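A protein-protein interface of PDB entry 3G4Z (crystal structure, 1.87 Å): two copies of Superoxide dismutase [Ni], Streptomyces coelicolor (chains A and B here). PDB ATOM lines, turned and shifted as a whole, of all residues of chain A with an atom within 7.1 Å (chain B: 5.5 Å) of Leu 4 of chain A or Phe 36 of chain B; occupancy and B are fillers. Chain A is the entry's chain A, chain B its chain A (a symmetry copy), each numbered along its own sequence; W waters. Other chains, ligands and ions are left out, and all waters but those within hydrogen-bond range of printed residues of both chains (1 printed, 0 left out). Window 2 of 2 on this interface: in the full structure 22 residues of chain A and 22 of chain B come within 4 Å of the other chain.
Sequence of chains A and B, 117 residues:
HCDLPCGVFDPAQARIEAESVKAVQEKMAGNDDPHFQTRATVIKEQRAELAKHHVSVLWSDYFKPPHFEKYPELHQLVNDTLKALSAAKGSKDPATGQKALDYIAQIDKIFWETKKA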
ATOM      1  N   HIS A   1     -35.917 -24.222  10.364  1.00  0.00           N
ATOM      2  CA  HIS A   1     -36.122 -25.689  10.162  1.00  0.00           C
ATOM      3  C   HIS A   1     -35.092 -26.280   9.202  1.00  0.00           C
ATOM      4  O   HIS A   1     -35.079 -27.486   8.947  1.00  0.00           O
ATOM      5  CB  HIS A   1     -37.538 -25.959   9.669  1.00  0.00           C
ATOM      6  CG  HIS A   1     -37.936 -25.118   8.501  1.00  0.00           C
ATOM      7  ND1 HIS A   1     -39.133 -24.442   8.446  1.00  0.00           N
ATOM      8  CD2 HIS A   1     -37.289 -24.833   7.346  1.00  0.00           C
ATOM      9  CE1 HIS A   1     -39.212 -23.784   7.304  1.00  0.00           C
ATOM     10  NE2 HIS A   1     -38.106 -24.005   6.616  1.00  0.00           N
ATOM     11  N   CYS A   2     -34.221 -25.407   8.700  1.00  0.00           N
ATOM     12  CA  CYS A   2     -33.144 -25.741   7.758  1.00  0.00           C
ATOM     13  C   CYS A   2     -31.773 -25.946   8.437  1.00  0.00           C
ATOM     14  O   CYS A   2     -30.845 -26.456   7.810  1.00  0.00           O
ATOM     15  CB  CYS A   2     -33.022 -24.604   6.758  1.00  0.00           C
ATOM     16  SG  CYS A   2     -32.764 -22.999   7.593  1.00  0.00           S
ATOM     17  N   ASP A   3     -31.649 -25.520   9.700  1.00  0.00           N
ATOM     18  CA  ASP A   3     -30.479 -25.824  10.565  1.00  0.00           C
ATOM     19  C   ASP A   3     -29.305 -24.817  10.454  1.00  0.00           C
ATOM     20  O   ASP A   3     -28.209 -25.087  10.973  1.00  0.00           O
ATOM     21  CB  ASP A   3     -29.985 -27.271  10.331  1.00  0.00           C
ATOM     22  CG  ASP A   3     -29.576 -27.982  11.616  1.00  0.00           C
ATOM     23  OD1 ASP A   3     -29.563 -27.361  12.692  1.00  0.00           O
ATOM     24  OD2 ASP A   3     -29.268 -29.192  11.538  1.00  0.00           O
ATOM     25  N   LEU A   4     -29.550 -23.664   9.806  1.00  0.00           N
ATOM     26  CA  LEU A   4     -28.497 -22.635   9.577  1.00  0.00           C
ATOM     27  C   LEU A   4     -27.763 -22.108  10.845  1.00  0.00           C
ATOM     28  O   LEU A   4     -26.533 -22.174  10.905  1.00  0.00           O
ATOM     29  CB  LEU A   4     -28.997 -21.471   8.678  1.00  0.00           C
ATOM     30  CG  LEU A   4     -28.006 -20.309   8.458  1.00  0.00           C
ATOM     31  CD1 LEU A   4     -26.721 -20.740   7.740  1.00  0.00           C
ATOM     32  CD2 LEU A   4     -28.664 -19.192   7.711  1.00  0.00           C
ATOM     33  N   PRO A   5     -28.503 -21.611  11.861  1.00  0.00           N
ATOM     34  CA  PRO A   5     -29.956 -21.550  12.016  1.00  0.00           C
ATOM     35  C   PRO A   5     -30.568 -20.385  11.224  1.00  0.00           C
ATOM     36  O   PRO A   5     -29.906 -19.360  11.022  1.00  0.00           O
ATOM     37  CB  PRO A   5     -30.147 -21.348  13.534  1.00  0.00           C
ATOM     38  CG  PRO A   5     -28.755 -21.140  14.128  1.00  0.00           C
ATOM     39  CD  PRO A   5     -27.812 -20.949  12.986  1.00  0.00           C
ATOM     40  N   CYS A   6     -31.802 -20.569  10.751  1.00  0.00           N
ATOM     41  CA  CYS A   6     -32.579 -19.488  10.139  1.00  0.00           C
ATOM     42  C   CYS A   6     -33.631 -18.948  11.124  1.00  0.00           C
ATOM     43  O   CYS A   6     -34.133 -17.832  10.948  1.00  0.00           O
ATOM     44  CB  CYS A   6     -33.282 -19.974   8.859  1.00  0.00           C
ATOM     45  SG  CYS A   6     -34.880 -20.863   9.148  1.00  0.00           S
ATOM     46  N   GLY A   7     -33.973 -19.749  12.138  1.00  0.00           N
ATOM     47  CA  GLY A   7     -34.989 -19.367  13.139  1.00  0.00           C
ATOM     48  C   GLY A   7     -36.460 -19.341  12.696  1.00  0.00           C
ATOM     49  O   GLY A   7     -37.300 -18.719  13.373  1.00  0.00           O
ATOM     50  N   ASP A  61     -34.044 -28.830  16.786  1.00  0.00           N
ATOM     51  CA  ASP A  61     -33.565 -27.549  16.236  1.00  0.00           C
ATOM     52  C   ASP A  61     -34.244 -26.289  16.770  1.00  0.00           C
ATOM     53  O   ASP A  61     -33.621 -25.243  16.767  1.00  0.00           O
ATOM     54  CB  ASP A  61     -33.632 -27.541  14.719  1.00  0.00           C
ATOM     55  CG  ASP A  61     -32.713 -28.560  14.094  1.00  0.00           C
ATOM     56  OD1 ASP A  61     -32.219 -29.466  14.788  1.00  0.00           O
ATOM     57  OD2 ASP A  61     -32.511 -28.463  12.872  1.00  0.00           O
ATOM     58  N   VAL B  24     -32.711 -16.388   5.772  1.00  0.00           N
ATOM     59  CA  VAL B  24     -31.318 -16.769   5.490  1.00  0.00           C
ATOM     60  C   VAL B  24     -30.585 -15.574   4.815  1.00  0.00           C
ATOM     61  O   VAL B  24     -29.450 -15.231   5.186  1.00  0.00           O
ATOM     62  CB  VAL B  24     -31.201 -18.045   4.631  1.00  0.00           C
ATOM     63  CG1 VAL B  24     -29.774 -18.151   4.025  1.00  0.00           C
ATOM     64  CG2 VAL B  24     -31.584 -19.347   5.468  1.00  0.00           C
ATOM     65  N   LYS B  27     -29.585 -13.159   7.406  1.00  0.00           N
ATOM     66  CA  LYS B  27     -28.449 -13.603   8.250  1.00  0.00           C
ATOM     67  C   LYS B  27     -27.126 -13.385   7.528  1.00  0.00           C
ATOM     68  O   LYS B  27     -26.091 -13.134   8.170  1.00  0.00           O
ATOM     69  CB  LYS B  27     -28.500 -15.099   8.599  1.00  0.00           C
ATOM     70  CG  LYS B  27     -29.762 -15.607   9.285  1.00  0.00           C
ATOM     71  CD  LYS B  27     -29.594 -15.640  10.778  1.00  0.00           C
ATOM     72  CE  LYS B  27     -30.908 -15.951  11.486  1.00  0.00           C
ATOM     73  NZ  LYS B  27     -30.795 -15.336  12.852  1.00  0.00           N
ATOM     74  N   MET B  28     -27.153 -13.566   6.213  1.00  0.00           N
ATOM     75  CA  MET B  28     -25.971 -13.363   5.393  1.00  0.00           C
ATOM     76  C   MET B  28     -25.354 -11.955   5.521  1.00  0.00           C
ATOM     77  O   MET B  28     -24.136 -11.810   5.392  1.00  0.00           O
ATOM     78  CB  MET B  28     -26.278 -13.718   3.946  1.00  0.00           C
ATOM     79  CG  MET B  28     -26.575 -15.248   3.800  1.00  0.00           C
ATOM     80  SD  MET B  28     -26.876 -15.709   2.106  1.00  0.00           S
ATOM     81  CE  MET B  28     -25.186 -15.966   1.499  1.00  0.00           C
ATOM     82  N   ASN B  31     -23.002 -11.864   9.201  1.00  0.00           N
ATOM     83  CA  ASN B  31     -21.836 -12.681   9.544  1.00  0.00           C
ATOM     84  C   ASN B  31     -21.044 -13.012   8.281  1.00  0.00           C
ATOM     85  O   ASN B  31     -21.527 -13.738   7.412  1.00  0.00           O
ATOM     86  CB  ASN B  31     -22.329 -13.954  10.271  1.00  0.00           C
ATOM     87  CG  ASN B  31     -21.208 -14.892  10.711  1.00  0.00           C
ATOM     88  OD1 ASN B  31     -20.011 -14.665  10.463  1.00  0.00           O
ATOM     89  ND2 ASN B  31     -21.608 -15.978  11.373  1.00  0.00           N
ATOM     90  N   ASP B  33     -18.238 -14.719   7.885  1.00  0.00           N
ATOM     91  CA  ASP B  33     -17.507 -15.981   7.838  1.00  0.00           C
ATOM     92  C   ASP B  33     -17.790 -16.676   6.490  1.00  0.00           C
ATOM     93  O   ASP B  33     -18.952 -16.880   6.156  1.00  0.00           O
ATOM     94  CB  ASP B  33     -17.967 -16.851   8.991  1.00  0.00           C
ATOM     95  CG  ASP B  33     -17.177 -18.130   9.097  1.00  0.00           C
ATOM     96  OD1 ASP B  33     -17.775 -19.217   9.192  1.00  0.00           O
ATOM     97  OD2 ASP B  33     -15.949 -18.038   9.064  1.00  0.00           O
ATOM     98  N   PRO B  34     -16.753 -16.988   5.681  1.00  0.00           N
ATOM     99  CA  PRO B  34     -17.041 -17.690   4.419  1.00  0.00           C
ATOM    100  C   PRO B  34     -17.757 -19.040   4.609  1.00  0.00           C
ATOM    101  O   PRO B  34     -18.603 -19.399   3.801  1.00  0.00           O
ATOM    102  CB  PRO B  34     -15.646 -17.925   3.813  1.00  0.00           C
ATOM    103  CG  PRO B  34     -14.801 -16.871   4.414  1.00  0.00           C
ATOM    104  CD  PRO B  34     -15.308 -16.689   5.818  1.00  0.00           C
ATOM    105  N   HIS B  35     -17.417 -19.767   5.666  1.00  0.00           N
ATOM    106  CA  HIS B  35     -18.074 -21.050   5.944  1.00  0.00           C
ATOM    107  C   HIS B  35     -19.561 -20.859   6.212  1.00  0.00           C
ATOM    108  O   HIS B  35     -20.400 -21.627   5.728  1.00  0.00           O
ATOM    109  CB  HIS B  35     -17.431 -21.734   7.121  1.00  0.00           C
ATOM    110  CG  HIS B  35     -17.978 -23.093   7.387  1.00  0.00           C
ATOM    111  ND1 HIS B  35     -18.501 -23.453   8.607  1.00  0.00           N
ATOM    112  CD2 HIS B  35     -18.102 -24.179   6.582  1.00  0.00           C
ATOM    113  CE1 HIS B  35     -18.889 -24.716   8.564  1.00  0.00           C
ATOM    114  NE2 HIS B  35     -18.669 -25.181   7.346  1.00  0.00           N
ATOM    115  N   PHE B  36     -19.877 -19.840   6.998  1.00  0.00           N
ATOM    116  CA  PHE B  36     -21.259 -19.478   7.264  1.00  0.00           C
ATOM    117  C   PHE B  36     -21.945 -19.032   5.971  1.00  0.00           C
ATOM    118  O   PHE B  36     -23.060 -19.492   5.666  1.00  0.00           O
ATOM    119  CB  PHE B  36     -21.343 -18.367   8.314  1.00  0.00           C
ATOM    120  CG  PHE B  36     -22.744 -17.929   8.610  1.00  0.00           C
ATOM    121  CD1 PHE B  36     -23.302 -16.850   7.935  1.00  0.00           C
ATOM    122  CD2 PHE B  36     -23.519 -18.617   9.537  1.00  0.00           C
ATOM    123  CE1 PHE B  36     -24.618 -16.443   8.179  1.00  0.00           C
ATOM    124  CE2 PHE B  36     -24.841 -18.211   9.799  1.00  0.00           C
ATOM    125  CZ  PHE B  36     -25.387 -17.118   9.108  1.00  0.00           C
ATOM    126  N   GLN B  37     -21.286 -18.165   5.190  1.00  0.00           N
ATOM    127  CA  GLN B  37     -21.867 -17.746   3.901  1.00  0.00           C
ATOM    128  C   GLN B  37     -22.206 -18.935   2.995  1.00  0.00           C
ATOM    129  O   GLN B  37     -23.243 -18.955   2.343  1.00  0.00           O
ATOM    130  CB  GLN B  37     -20.930 -16.770   3.165  1.00  0.00           C
ATOM    131  CG  GLN B  37     -20.707 -15.518   3.928  1.00  0.00           C
ATOM    132  CD  GLN B  37     -21.859 -14.533   3.814  1.00  0.00           C
ATOM    133  OE1 GLN B  37     -22.333 -14.238   2.719  1.00  0.00           O
ATOM    134  NE2 GLN B  37     -22.281 -13.989   4.941  1.00  0.00           N
ATOM    135  N   THR B  38     -21.333 -19.939   2.996  1.00  0.00           N
ATOM    136  CA  THR B  38     -21.527 -21.087   2.144  1.00  0.00           C
ATOM    137  C   THR B  38     -22.694 -21.915   2.686  1.00  0.00           C
ATOM    138  O   THR B  38     -23.572 -22.275   1.919  1.00  0.00           O
ATOM    139  CB  THR B  38     -20.225 -21.885   2.021  1.00  0.00           C
ATOM    140  OG1 THR B  38     -19.243 -21.057   1.350  1.00  0.00           O
ATOM    141  CG2 THR B  38     -20.441 -23.179   1.238  1.00  0.00           C
ATOM    142  N   ARG B  39     -22.722 -22.192   4.001  1.00  0.00           N
ATOM    143  CA  ARG B  39     -23.884 -22.931   4.548  1.00  0.00           C
ATOM    144  C   ARG B  39     -25.217 -22.201   4.277  1.00  0.00           C
ATOM    145  O   ARG B  39     -26.222 -22.857   3.928  1.00  0.00           O
ATOM    146  CB  ARG B  39     -23.718 -23.238   6.052  1.00  0.00           C
ATOM    147  CG  ARG B  39     -22.504 -24.104   6.400  1.00  0.00           C
ATOM    148  CD  ARG B  39     -22.468 -24.465   7.923  1.00  0.00           C
ATOM    149  NE  ARG B  39     -23.773 -25.042   8.256  1.00  0.00           N
ATOM    150  CZ  ARG B  39     -24.680 -24.500   9.071  1.00  0.00           C
ATOM    151  NH1 ARG B  39     -24.405 -23.403   9.754  1.00  0.00           N
ATOM    152  NH2 ARG B  39     -25.849 -25.091   9.223  1.00  0.00           N
ATOM    153  N   ALA B  40     -25.239 -20.866   4.455  1.00  0.00           N
ATOM    154  CA  ALA B  40     -26.430 -20.066   4.174  1.00  0.00           C
ATOM    155  C   ALA B  40     -26.824 -20.300   2.728  1.00  0.00           C
ATOM    156  O   ALA B  40     -28.032 -20.413   2.420  1.00  0.00           O
ATOM    157  CB  ALA B  40     -26.191 -18.565   4.418  1.00  0.00           C
ATOM    158  N   THR B  41     -25.815 -20.339   1.842  1.00  0.00           N
ATOM    159  CA  THR B  41     -26.079 -20.529   0.386  1.00  0.00           C
ATOM    160  C   THR B  41     -26.692 -21.903   0.124  1.00  0.00           C
ATOM    161  O   THR B  41     -27.712 -22.001  -0.547  1.00  0.00           O
ATOM    162  CB  THR B  41     -24.816 -20.279  -0.491  1.00  0.00           C
ATOM    163  OG1 THR B  41     -24.304 -18.979  -0.200  1.00  0.00           O
ATOM    164  CG2 THR B  41     -25.157 -20.334  -1.963  1.00  0.00           C
ATOM    165  N   ILE B  43     -28.390 -23.766   2.178  1.00  0.00           N
ATOM    166  CA  ILE B  43     -29.697 -23.873   2.815  1.00  0.00           C
ATOM    167  C   ILE B  43     -30.699 -23.077   2.015  1.00  0.00           C
ATOM    168  O   ILE B  43     -31.833 -23.534   1.741  1.00  0.00           O
ATOM    169  CB  ILE B  43     -29.630 -23.422   4.266  1.00  0.00           C
ATOM    170  CG1 ILE B  43     -28.813 -24.465   5.027  1.00  0.00           C
ATOM    171  CG2 ILE B  43     -31.049 -23.231   4.869  1.00  0.00           C
ATOM    172  CD1 ILE B  43     -28.427 -24.089   6.387  1.00  0.00           C
HETATM  173  O   HOH W   1     -26.126 -25.541  12.635  1.00  0.00           O
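NH2 of Arg 39 of chain B is in hydrogen-bond range of O of Asp 3 of chain A (2.9 Å). O of Leu 4 of chain A lies within hydrogen-bond range of NH1 of Arg 39 of chain B (2.7 Å).
The side-chain carboxylate (OD1) of Asp 33 of chain B is in hydrogen-bond range of the backbone NH (N) of Phe 36 of chain B, 3.1 Å away.
Cys 2 of chain A touches Ile 43 of chain B. Leu 4 of chain A touches Val 24 of chain B. Phe 36 of chain B touches Leu 4 of chain A. CD1 of Leu 4 of chain A touches N of Ala 40 of chain B (3.6 Å). CD1 of Ile 43 of chain B touches CA of Leu 4 of chain A (3.5 Å). Lys 27 of chain B touches Pro 5 of chain A. Val 24 of chain B touches Cys 6 of chain A (CG2 to CB, 3.8 Å). Cys 6 of chain A touches Lys 27 of chain B (O to CE, 3.8 Å).
Of the printed residues of chain B, Asp 3 of chain A touches Arg 39. Leu 4 of chain A touches just these residues of chain B: Val 24 (3.7 Å), Phe 36 (3.8 Å), Arg 39 (2.7 Å), Ala 40 (3.6 Å) and Ile 43 (3.5 Å). Of the printed residues of chain B, Cys 6 of chain A touches Val 24 (3.8 Å) and Lys 27 (3.8 Å). Gly 7 of chain A touches none of the printed residues of chain B. Of the printed residues of chain A, Val 24 of chain B touches Leu 4 (3.7 Å) and Cys 6 (3.8 Å). Asp 33 of chain B touches none of the printed residues of chain A. Phe 36 of chain B touches one residue of chain A. Of the printed residues of chain A, Arg 39 of chain B touches Asp 3 and Leu 4. Printed residues of chain A within 4 Å of Ala 40 of chain B: Leu 4. The nearest printed residue of chain B that does not touch Cys 6 of chain A is Ile 43 of chain B (5.6 Å).
Of the 14 printed residues of chain B, 6 touch a printed residue of chain A. Along chain B the printed residues that touch a printed residue of chain A span positions 24 to 43. Hydrophobic or aromatic side chains of chain A that line the printed part of chain B: Leu 4. Among the printed residues, no Asp or Glu carboxylate lies within 4 Å of a Lys or Arg side-chain nitrogen of the other chain.
No position is printed for both chains.
Water W1 bridges O of Asp 3 of chain A (2.7 Å) and NH2 of Arg 39 of chain B (3.5 Å).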
